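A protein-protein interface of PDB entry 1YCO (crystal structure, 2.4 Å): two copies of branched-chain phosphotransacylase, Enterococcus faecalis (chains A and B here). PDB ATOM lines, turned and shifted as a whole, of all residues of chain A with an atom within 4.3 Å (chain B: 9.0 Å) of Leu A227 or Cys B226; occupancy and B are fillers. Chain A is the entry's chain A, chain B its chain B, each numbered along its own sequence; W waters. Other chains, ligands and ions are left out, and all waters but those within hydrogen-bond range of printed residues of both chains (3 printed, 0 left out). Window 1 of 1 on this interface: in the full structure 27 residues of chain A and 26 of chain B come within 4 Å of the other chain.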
ATOM      1  N   LEU A 116      17.480 -15.959  18.240  1.00  0.00           N
ATOM      2  CA  LEU A 116      16.099 -15.519  18.228  1.00  0.00           C
ATOM      3  C   LEU A 116      16.146 -14.025  18.484  1.00  0.00           C
ATOM      4  O   LEU A 116      16.823 -13.567  19.410  1.00  0.00           O
ATOM      5  CB  LEU A 116      15.306 -16.197  19.346  1.00  0.00           C
ATOM      6  CG  LEU A 116      13.848 -15.743  19.547  1.00  0.00           C
ATOM      7  CD1 LEU A 116      13.036 -15.942  18.283  1.00  0.00           C
ATOM      8  CD2 LEU A 116      13.244 -16.530  20.700  1.00  0.00           C
ATOM      9  N   LEU A 191       7.539 -21.478  11.621  1.00  0.00           N
ATOM     10  CA  LEU A 191       8.520 -22.003  12.571  1.00  0.00           C
ATOM     11  C   LEU A 191       9.036 -23.404  12.222  1.00  0.00           C
ATOM     12  O   LEU A 191      10.235 -23.655  12.255  1.00  0.00           O
ATOM     13  CB  LEU A 191       7.919 -22.011  13.990  1.00  0.00           C
ATOM     14  CG  LEU A 191       8.792 -22.490  15.158  1.00  0.00           C
ATOM     15  CD1 LEU A 191       9.851 -21.445  15.465  1.00  0.00           C
ATOM     16  CD2 LEU A 191       7.928 -22.740  16.400  1.00  0.00           C
ATOM     17  N   VAL A 223       5.279 -12.749  20.039  1.00  0.00           N
ATOM     18  CA  VAL A 223       5.690 -13.978  19.395  1.00  0.00           C
ATOM     19  C   VAL A 223       7.038 -14.446  19.977  1.00  0.00           C
ATOM     20  O   VAL A 223       7.160 -15.565  20.471  1.00  0.00           O
ATOM     21  CB  VAL A 223       5.787 -13.762  17.866  1.00  0.00           C
ATOM     22  CG1 VAL A 223       6.271 -15.019  17.172  1.00  0.00           C
ATOM     23  CG2 VAL A 223       4.422 -13.349  17.323  1.00  0.00           C
ATOM     24  N   GLY A 224       8.044 -13.581  19.935  1.00  0.00           N
ATOM     25  CA  GLY A 224       9.347 -13.939  20.465  1.00  0.00           C
ATOM     26  C   GLY A 224       9.351 -14.363  21.927  1.00  0.00           C
ATOM     27  O   GLY A 224      10.039 -15.318  22.312  1.00  0.00           O
ATOM     28  N   ASN A 225       8.592 -13.640  22.746  1.00  0.00           N
ATOM     29  CA  ASN A 225       8.480 -13.926  24.175  1.00  0.00           C
ATOM     30  C   ASN A 225       7.863 -15.300  24.392  1.00  0.00           C
ATOM     31  O   ASN A 225       8.382 -16.117  25.147  1.00  0.00           O
ATOM     32  CB  ASN A 225       7.593 -12.883  24.877  1.00  0.00           C
ATOM     33  CG  ASN A 225       7.365 -13.197  26.358  1.00  0.00           C
ATOM     34  OD1 ASN A 225       8.187 -12.859  27.199  1.00  0.00           O
ATOM     35  ND2 ASN A 225       6.250 -13.856  26.671  1.00  0.00           N
ATOM     36  N   CYS A 226       6.747 -15.542  23.720  1.00  0.00           N
ATOM     37  CA  CYS A 226       6.047 -16.804  23.856  1.00  0.00           C
ATOM     38  C   CYS A 226       6.903 -17.974  23.390  1.00  0.00           C
ATOM     39  O   CYS A 226       6.914 -19.017  24.024  1.00  0.00           O
ATOM     40  CB  CYS A 226       4.741 -16.752  23.072  1.00  0.00           C
ATOM     41  SG  CYS A 226       3.550 -18.027  23.532  1.00  0.00           S
ATOM     42  N   LEU A 227       7.630 -17.789  22.292  1.00  0.00           N
ATOM     43  CA  LEU A 227       8.486 -18.826  21.766  1.00  0.00           C
ATOM     44  C   LEU A 227       9.619 -19.065  22.772  1.00  0.00           C
ATOM     45  O   LEU A 227       9.945 -20.202  23.121  1.00  0.00           O
ATOM     46  CB  LEU A 227       9.066 -18.382  20.422  1.00  0.00           C
ATOM     47  CG  LEU A 227       9.901 -19.399  19.629  1.00  0.00           C
ATOM     48  CD1 LEU A 227       9.057 -20.656  19.346  1.00  0.00           C
ATOM     49  CD2 LEU A 227      10.344 -18.770  18.317  1.00  0.00           C
ATOM     50  N   TYR A 228      10.206 -17.964  23.233  1.00  0.00           N
ATOM     51  CA  TYR A 228      11.288 -17.983  24.201  1.00  0.00           C
ATOM     52  C   TYR A 228      10.911 -18.843  25.410  1.00  0.00           C
ATOM     53  O   TYR A 228      11.579 -19.830  25.706  1.00  0.00           O
ATOM     54  CB  TYR A 228      11.574 -16.547  24.660  1.00  0.00           C
ATOM     55  CG  TYR A 228      12.793 -16.357  25.534  1.00  0.00           C
ATOM     56  CD1 TYR A 228      13.932 -15.721  25.038  1.00  0.00           C
ATOM     57  CD2 TYR A 228      12.802 -16.788  26.858  1.00  0.00           C
ATOM     58  CE1 TYR A 228      15.053 -15.513  25.846  1.00  0.00           C
ATOM     59  CE2 TYR A 228      13.915 -16.592  27.678  1.00  0.00           C
ATOM     60  CZ  TYR A 228      15.039 -15.952  27.169  1.00  0.00           C
ATOM     61  OH  TYR A 228      16.145 -15.757  27.979  1.00  0.00           O
ATOM     62  N   LYS A 229       9.831 -18.462  26.089  1.00  0.00           N
ATOM     63  CA  LYS A 229       9.367 -19.162  27.284  1.00  0.00           C
ATOM     64  C   LYS A 229       8.960 -20.598  27.017  1.00  0.00           C
ATOM     65  O   LYS A 229       9.209 -21.490  27.829  1.00  0.00           O
ATOM     66  CB  LYS A 229       8.189 -18.415  27.922  1.00  0.00           C
ATOM     67  CG  LYS A 229       8.531 -16.999  28.390  1.00  0.00           C
ATOM     68  CD  LYS A 229       7.430 -16.416  29.279  1.00  0.00           C
ATOM     69  CE  LYS A 229       7.532 -14.891  29.425  1.00  0.00           C
ATOM     70  NZ  LYS A 229       8.861 -14.410  29.911  1.00  0.00           N
ATOM     71  N   SER A 230       8.320 -20.810  25.878  1.00  0.00           N
ATOM     72  CA  SER A 230       7.887 -22.130  25.500  1.00  0.00           C
ATOM     73  C   SER A 230       9.099 -23.059  25.331  1.00  0.00           C
ATOM     74  O   SER A 230       9.049 -24.233  25.715  1.00  0.00           O
ATOM     75  CB  SER A 230       7.084 -22.049  24.206  1.00  0.00           C
ATOM     76  OG  SER A 230       6.841 -23.340  23.688  1.00  0.00           O
ATOM     77  N   LEU A 231      10.185 -22.526  24.773  1.00  0.00           N
ATOM     78  CA  LEU A 231      11.400 -23.304  24.561  1.00  0.00           C
ATOM     79  C   LEU A 231      12.007 -23.786  25.873  1.00  0.00           C
ATOM     80  O   LEU A 231      12.374 -24.947  25.998  1.00  0.00           O
ATOM     81  CB  LEU A 231      12.439 -22.480  23.790  1.00  0.00           C
ATOM     82  CG  LEU A 231      12.084 -22.208  22.331  1.00  0.00           C
ATOM     83  CD1 LEU A 231      13.091 -21.240  21.710  1.00  0.00           C
ATOM     84  CD2 LEU A 231      12.038 -23.525  21.574  1.00  0.00           C
ATOM     85  N   LEU B 116      -5.789 -24.216  23.792  1.00  0.00           N
ATOM     86  CA  LEU B 116      -5.126 -23.094  23.161  1.00  0.00           C
ATOM     87  C   LEU B 116      -6.090 -22.579  22.125  1.00  0.00           C
ATOM     88  O   LEU B 116      -6.464 -23.305  21.196  1.00  0.00           O
ATOM     89  CB  LEU B 116      -3.835 -23.541  22.475  1.00  0.00           C
ATOM     90  CG  LEU B 116      -3.058 -22.445  21.744  1.00  0.00           C
ATOM     91  CD1 LEU B 116      -2.727 -21.318  22.721  1.00  0.00           C
ATOM     92  CD2 LEU B 116      -1.798 -23.019  21.146  1.00  0.00           C
ATOM     93  N   ASP B 118      -7.429 -20.116  19.093  1.00  0.00           N
ATOM     94  CA  ASP B 118      -7.265 -19.337  17.894  1.00  0.00           C
ATOM     95  C   ASP B 118      -5.889 -19.171  17.312  1.00  0.00           C
ATOM     96  O   ASP B 118      -5.270 -18.120  17.414  1.00  0.00           O
ATOM     97  CB  ASP B 118      -7.954 -17.999  18.044  1.00  0.00           C
ATOM     98  CG  ASP B 118      -8.784 -17.683  16.832  1.00  0.00           C
ATOM     99  OD1 ASP B 118      -8.985 -18.613  16.027  1.00  0.00           O
ATOM    100  OD2 ASP B 118      -9.231 -16.536  16.674  1.00  0.00           O
ATOM    101  N   CYS B 119      -5.447 -20.236  16.652  1.00  0.00           N
ATOM    102  CA  CYS B 119      -4.149 -20.285  15.989  1.00  0.00           C
ATOM    103  C   CYS B 119      -4.413 -20.385  14.498  1.00  0.00           C
ATOM    104  O   CYS B 119      -3.503 -20.679  13.721  1.00  0.00           O
ATOM    105  CB  CYS B 119      -3.373 -21.531  16.421  1.00  0.00           C
ATOM    106  SG  CYS B 119      -3.479 -21.956  18.167  1.00  0.00           S
ATOM    107  N   ALA B 120      -5.654 -20.143  14.087  1.00  0.00           N
ATOM    108  CA  ALA B 120      -5.983 -20.262  12.669  1.00  0.00           C
ATOM    109  C   ALA B 120      -7.014 -19.286  12.118  1.00  0.00           C
ATOM    110  O   ALA B 120      -6.830 -18.747  11.028  1.00  0.00           O
ATOM    111  CB  ALA B 120      -6.433 -21.687  12.390  1.00  0.00           C
ATOM    112  N   ALA B 156       3.092 -10.431  26.665  1.00  0.00           N
ATOM    113  CA  ALA B 156       4.495 -10.334  27.016  1.00  0.00           C
ATOM    114  C   ALA B 156       4.714  -9.115  27.906  1.00  0.00           C
ATOM    115  O   ALA B 156       5.830  -8.851  28.369  1.00  0.00           O
ATOM    116  CB  ALA B 156       5.336 -10.224  25.757  1.00  0.00           C
ATOM    117  N   LEU B 191       3.317 -16.434  29.674  1.00  0.00           N
ATOM    118  CA  LEU B 191       3.170 -17.870  29.521  1.00  0.00           C
ATOM    119  C   LEU B 191       3.544 -18.689  30.761  1.00  0.00           C
ATOM    120  O   LEU B 191       2.763 -19.524  31.220  1.00  0.00           O
ATOM    121  CB  LEU B 191       3.975 -18.355  28.319  1.00  0.00           C
ATOM    122  CG  LEU B 191       3.728 -19.802  27.892  1.00  0.00           C
ATOM    123  CD1 LEU B 191       2.254 -20.019  27.652  1.00  0.00           C
ATOM    124  CD2 LEU B 191       4.533 -20.096  26.637  1.00  0.00           C
ATOM    125  N   VAL B 218      -4.482 -16.370  22.942  1.00  0.00           N
ATOM    126  CA  VAL B 218      -3.444 -15.542  22.344  1.00  0.00           C
ATOM    127  C   VAL B 218      -3.992 -14.233  21.777  1.00  0.00           C
ATOM    128  O   VAL B 218      -5.193 -14.110  21.521  1.00  0.00           O
ATOM    129  CB  VAL B 218      -2.717 -16.310  21.222  1.00  0.00           C
ATOM    130  CG1 VAL B 218      -1.848 -17.393  21.819  1.00  0.00           C
ATOM    131  CG2 VAL B 218      -3.745 -16.940  20.258  1.00  0.00           C
ATOM    132  N   THR B 220      -2.898 -12.763  18.872  1.00  0.00           N
ATOM    133  CA  THR B 220      -2.963 -12.888  17.423  1.00  0.00           C
ATOM    134  C   THR B 220      -2.688 -14.334  17.009  1.00  0.00           C
ATOM    135  O   THR B 220      -2.271 -15.151  17.829  1.00  0.00           O
ATOM    136  CB  THR B 220      -1.900 -11.974  16.747  1.00  0.00           C
ATOM    137  OG1 THR B 220      -0.582 -12.465  17.037  1.00  0.00           O
ATOM    138  CG2 THR B 220      -2.011 -10.540  17.259  1.00  0.00           C
ATOM    139  N   ILE B 221      -2.920 -14.652  15.738  1.00  0.00           N
ATOM    140  CA  ILE B 221      -2.650 -16.006  15.266  1.00  0.00           C
ATOM    141  C   ILE B 221      -1.140 -16.227  15.210  1.00  0.00           C
ATOM    142  O   ILE B 221      -0.670 -17.361  15.307  1.00  0.00           O
ATOM    143  CB  ILE B 221      -3.220 -16.274  13.854  1.00  0.00           C
ATOM    144  CG1 ILE B 221      -2.857 -15.099  12.946  1.00  0.00           C
ATOM    145  CG2 ILE B 221      -4.730 -16.540  13.919  1.00  0.00           C
ATOM    146  CD1 ILE B 221      -3.423 -15.199  11.555  1.00  0.00           C
ATOM    147  N   ASP B 222      -0.374 -15.156  15.047  1.00  0.00           N
ATOM    148  CA  ASP B 222       1.071 -15.318  15.000  1.00  0.00           C
ATOM    149  C   ASP B 222       1.598 -15.933  16.276  1.00  0.00           C
ATOM    150  O   ASP B 222       2.492 -16.781  16.235  1.00  0.00           O
ATOM    151  CB  ASP B 222       1.775 -13.988  14.736  1.00  0.00           C
ATOM    152  CG  ASP B 222       1.936 -13.715  13.249  1.00  0.00           C
ATOM    153  OD1 ASP B 222       2.361 -14.639  12.522  1.00  0.00           O
ATOM    154  OD2 ASP B 222       1.634 -12.592  12.798  1.00  0.00           O
ATOM    155  N   VAL B 223       1.038 -15.497  17.400  1.00  0.00           N
ATOM    156  CA  VAL B 223       1.409 -16.001  18.711  1.00  0.00           C
ATOM    157  C   VAL B 223       0.874 -17.428  18.898  1.00  0.00           C
ATOM    158  O   VAL B 223       1.598 -18.329  19.330  1.00  0.00           O
ATOM    159  CB  VAL B 223       0.841 -15.096  19.841  1.00  0.00           C
ATOM    160  CG1 VAL B 223       1.049 -15.760  21.210  1.00  0.00           C
ATOM    161  CG2 VAL B 223       1.537 -13.734  19.812  1.00  0.00           C
ATOM    162  N   GLY B 224      -0.400 -17.626  18.573  1.00  0.00           N
ATOM    163  CA  GLY B 224      -0.980 -18.948  18.711  1.00  0.00           C
ATOM    164  C   GLY B 224      -0.324 -19.983  17.811  1.00  0.00           C
ATOM    165  O   GLY B 224      -0.087 -21.127  18.202  1.00  0.00           O
ATOM    166  N   ASN B 225      -0.027 -19.579  16.587  1.00  0.00           N
ATOM    167  CA  ASN B 225       0.580 -20.494  15.649  1.00  0.00           C
ATOM    168  C   ASN B 225       1.967 -20.897  16.116  1.00  0.00           C
ATOM    169  O   ASN B 225       2.340 -22.070  16.073  1.00  0.00           O
ATOM    170  CB  ASN B 225       0.657 -19.846  14.275  1.00  0.00           C
ATOM    171  CG  ASN B 225       1.299 -20.742  13.258  1.00  0.00           C
ATOM    172  OD1 ASN B 225       2.513 -20.928  13.259  1.00  0.00           O
ATOM    173  ND2 ASN B 225       0.489 -21.314  12.384  1.00  0.00           N
ATOM    174  N   CYS B 226       2.717 -19.911  16.588  1.00  0.00           N
ATOM    175  CA  CYS B 226       4.065 -20.132  17.067  1.00  0.00           C
ATOM    176  C   CYS B 226       4.074 -21.079  18.274  1.00  0.00           C
ATOM    177  O   CYS B 226       4.794 -22.083  18.302  1.00  0.00           O
ATOM    178  CB  CYS B 226       4.687 -18.792  17.456  1.00  0.00           C
ATOM    179  SG  CYS B 226       6.482 -18.834  17.552  1.00  0.00           S
ATOM    180  N   LEU B 227       3.268 -20.741  19.270  1.00  0.00           N
ATOM    181  CA  LEU B 227       3.172 -21.543  20.466  1.00  0.00           C
ATOM    182  C   LEU B 227       2.723 -22.961  20.100  1.00  0.00           C
ATOM    183  O   LEU B 227       3.262 -23.949  20.597  1.00  0.00           O
ATOM    184  CB  LEU B 227       2.186 -20.906  21.428  1.00  0.00           C
ATOM    185  CG  LEU B 227       2.070 -21.616  22.764  1.00  0.00           C
ATOM    186  CD1 LEU B 227       3.442 -21.767  23.416  1.00  0.00           C
ATOM    187  CD2 LEU B 227       1.134 -20.809  23.644  1.00  0.00           C
ATOM    188  N   TYR B 228       1.735 -23.038  19.216  1.00  0.00           N
ATOM    189  CA  TYR B 228       1.207 -24.307  18.741  1.00  0.00           C
ATOM    190  C   TYR B 228       2.329 -25.198  18.159  1.00  0.00           C
ATOM    191  O   TYR B 228       2.483 -26.355  18.547  1.00  0.00           O
ATOM    192  CB  TYR B 228       0.154 -24.046  17.658  1.00  0.00           C
ATOM    193  CG  TYR B 228      -0.451 -25.296  17.085  1.00  0.00           C
ATOM    194  CD1 TYR B 228      -1.581 -25.869  17.665  1.00  0.00           C
ATOM    195  CD2 TYR B 228       0.117 -25.922  15.977  1.00  0.00           C
ATOM    196  CE1 TYR B 228      -2.135 -27.036  17.156  1.00  0.00           C
ATOM    197  CE2 TYR B 228      -0.426 -27.096  15.458  1.00  0.00           C
ATOM    198  CZ  TYR B 228      -1.556 -27.646  16.057  1.00  0.00           C
ATOM    199  OH  TYR B 228      -2.098 -28.817  15.570  1.00  0.00           O
ATOM    200  N   LYS B 229       3.116 -24.640  17.246  1.00  0.00           N
ATOM    201  CA  LYS B 229       4.182 -25.388  16.613  1.00  0.00           C
ATOM    202  C   LYS B 229       5.376 -25.702  17.494  1.00  0.00           C
ATOM    203  O   LYS B 229       5.986 -26.755  17.334  1.00  0.00           O
ATOM    204  CB  LYS B 229       4.643 -24.685  15.341  1.00  0.00           C
ATOM    205  CG  LYS B 229       3.591 -24.751  14.242  1.00  0.00           C
ATOM    206  CD  LYS B 229       4.127 -24.307  12.886  1.00  0.00           C
ATOM    207  CE  LYS B 229       3.109 -24.618  11.777  1.00  0.00           C
ATOM    208  NZ  LYS B 229       2.628 -26.055  11.809  1.00  0.00           N
ATOM    209  N   SER B 230       5.707 -24.809  18.425  1.00  0.00           N
ATOM    210  CA  SER B 230       6.830 -25.054  19.306  1.00  0.00           C
ATOM    211  C   SER B 230       6.491 -26.186  20.281  1.00  0.00           C
ATOM    212  O   SER B 230       7.357 -26.975  20.647  1.00  0.00           O
ATOM    213  CB  SER B 230       7.209 -23.792  20.093  1.00  0.00           C
ATOM    214  OG  SER B 230       6.209 -23.463  21.033  1.00  0.00           O
ATOM    215  N   LEU B 231       5.235 -26.271  20.696  1.00  0.00           N
ATOM    216  CA  LEU B 231       4.842 -27.323  21.612  1.00  0.00           C
ATOM    217  C   LEU B 231       4.955 -28.663  20.907  1.00  0.00           C
ATOM    218  O   LEU B 231       5.289 -29.675  21.516  1.00  0.00           O
ATOM    219  CB  LEU B 231       3.406 -27.110  22.087  1.00  0.00           C
ATOM    220  CG  LEU B 231       3.216 -25.888  22.991  1.00  0.00           C
ATOM    221  CD1 LEU B 231       1.737 -25.674  23.266  1.00  0.00           C
ATOM    222  CD2 LEU B 231       4.009 -26.072  24.278  1.00  0.00           C
ATOM    223  N   THR B 232       4.684 -28.653  19.613  1.00  0.00           N
ATOM    224  CA  THR B 232       4.745 -29.855  18.808  1.00  0.00           C
ATOM    225  C   THR B 232       6.169 -30.260  18.421  1.00  0.00           C
ATOM    226  O   THR B 232       6.572 -31.402  18.635  1.00  0.00           O
ATOM    227  CB  THR B 232       3.881 -29.669  17.553  1.00  0.00           C
ATOM    228  OG1 THR B 232       2.507 -29.855  17.910  1.00  0.00           O
ATOM    229  CG2 THR B 232       4.267 -30.650  16.477  1.00  0.00           C
ATOM    230  N   LEU B 233       6.927 -29.321  17.868  1.00  0.00           N
ATOM    231  CA  LEU B 233       8.297 -29.578  17.439  1.00  0.00           C
ATOM    232  C   LEU B 233       9.295 -29.899  18.548  1.00  0.00           C
ATOM    233  O   LEU B 233      10.026 -30.882  18.449  1.00  0.00           O
ATOM    234  CB  LEU B 233       8.825 -28.380  16.663  1.00  0.00           C
ATOM    235  CG  LEU B 233       8.112 -28.029  15.369  1.00  0.00           C
ATOM    236  CD1 LEU B 233       8.560 -26.634  14.914  1.00  0.00           C
ATOM    237  CD2 LEU B 233       8.423 -29.072  14.319  1.00  0.00           C
ATOM    238  N   PHE B 234       9.319 -29.066  19.589  1.00  0.00           N
ATOM    239  CA  PHE B 234      10.267 -29.221  20.693  1.00  0.00           C
ATOM    240  C   PHE B 234       9.683 -29.636  22.035  1.00  0.00           C
ATOM    241  O   PHE B 234      10.421 -30.063  22.925  1.00  0.00           O
ATOM    242  CB  PHE B 234      11.048 -27.918  20.894  1.00  0.00           C
ATOM    243  CG  PHE B 234      11.389 -27.210  19.615  1.00  0.00           C
ATOM    244  CD1 PHE B 234      10.664 -26.090  19.211  1.00  0.00           C
ATOM    245  CD2 PHE B 234      12.428 -27.663  18.809  1.00  0.00           C
ATOM    246  CE1 PHE B 234      10.971 -25.437  18.029  1.00  0.00           C
ATOM    247  CE2 PHE B 234      12.738 -27.015  17.626  1.00  0.00           C
ATOM    248  CZ  PHE B 234      12.008 -25.901  17.235  1.00  0.00           C
HETATM  249  O   HOH W   1       5.119 -19.810  13.124  1.00  0.00           O
HETATM  250  O   HOH W   2       8.275 -26.072  23.412  1.00  0.00           O
HETATM  251  O   HOH W   3       3.576 -13.379  24.978  1.00  0.00           O
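OG of Ser A230 is in hydrogen-bond range of OG of Ser B230 (2.7 Å).
The backbone carbonyl oxygen of Leu B227 lies within hydrogen-bond range of the side-chain hydroxyl of Ser B230 (3.0 Å).
The side-chain hydroxyl of Thr B220 is in hydrogen-bond range of the backbone NH of Val B223 (3.5 Å).
The side-chain hydroxyl (OG1) of Thr B220 sits close to the backbone NH (N) of Asp B222 (3.4 Å).
The side-chain amide oxygen of Asn A225 sits close to the side-chain amino group of Lys A229 (3.2 Å).
O of Cys B226 is in hydrogen-bond range of OG of Ser B230.
Among the printed residues, merely in contact across the chains: Asn A225 with Ala B156, Leu A227 with Cys B226, Leu A191 with Ser B230, Cys A226 with Leu B227, Cys A226 with Leu B191, Leu A227 with Ser B230, Leu A191 with Cys B226, Ser A230 with Leu B227, Leu A231 with Phe B234, Val A223 with Asp B222, Val A223 with Val B223, Val A223 with Cys B226, Ser A230 with Leu B191, Leu A191 with Lys B229 and Ser A230 with Leu B231.
Of chain B, only Leu B191 (3.7 Å) and Leu B227 (3.7 Å) come within 4 Å of Cys A226.
Leu A227 touches just these residues of chain B: Cys B226 (3.6 Å) and Ser B230 (3.7 Å).
Of chain B, only Leu B191 (3.9 Å), Leu B227 (3.7 Å), Ser B230 (2.7 Å) and Leu B231 (3.98 Å) come within 4 Å of Ser A230.
Cys B119 touches none of the printed residues of chain A.
Thr B220 touches none of the printed residues of chain A.
Printed residues of chain A within 4 Å of Val B223: Val A223 (3.8 Å).
Cys B226 touches just these residues of chain A: Leu A191, Val A223 and Leu A227.
Printed residues of chain A within 4 Å of Leu B227: Cys A226 (3.7 Å) and Ser A230 (3.7 Å).
Of the printed residues of chain A, Leu B231 touches Ser A230 (3.98 Å).
The nearest residue of chain B that does not touch Leu A227 is Phe B234 (5.3 Å).
Of the 11 printed residues of chain A, 7 touch a printed residue of chain B.
Of the 22 printed residues of chain B, 10 touch a printed residue of chain A.
Among the printed residues, no Asp or Glu carboxylate lies within 4 Å of a Lys or Arg side-chain nitrogen of the other chain.
Leu A191 touches Cys B226, and with the chains exchanged Cys A226 touches Leu B191.
Val A223 touches its own counterpart, Val B223.
Val A223 touches Cys B226, but with the chains exchanged Cys A226 does not touch Val B223 (4.1 Å).
Ser A230 touches Leu B231, but with the chains exchanged Leu A231 does not touch Ser B230 (5.1 Å).
11 positions are printed for both chains.
Water W1 lies within hydrogen-bond range of OD1 of Asn B225 (2.8 Å) and N of Leu A191 (3.3 Å).
Water W2 lies within hydrogen-bond range of O of Ser A230 and O of Ser B230.
Water W3 lies within hydrogen-bond range of the side-chain amide nitrogen (ND2) of Asn A225 (3.2 Å) and the backbone NH (N) of Ala B156 (3.4 Å).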
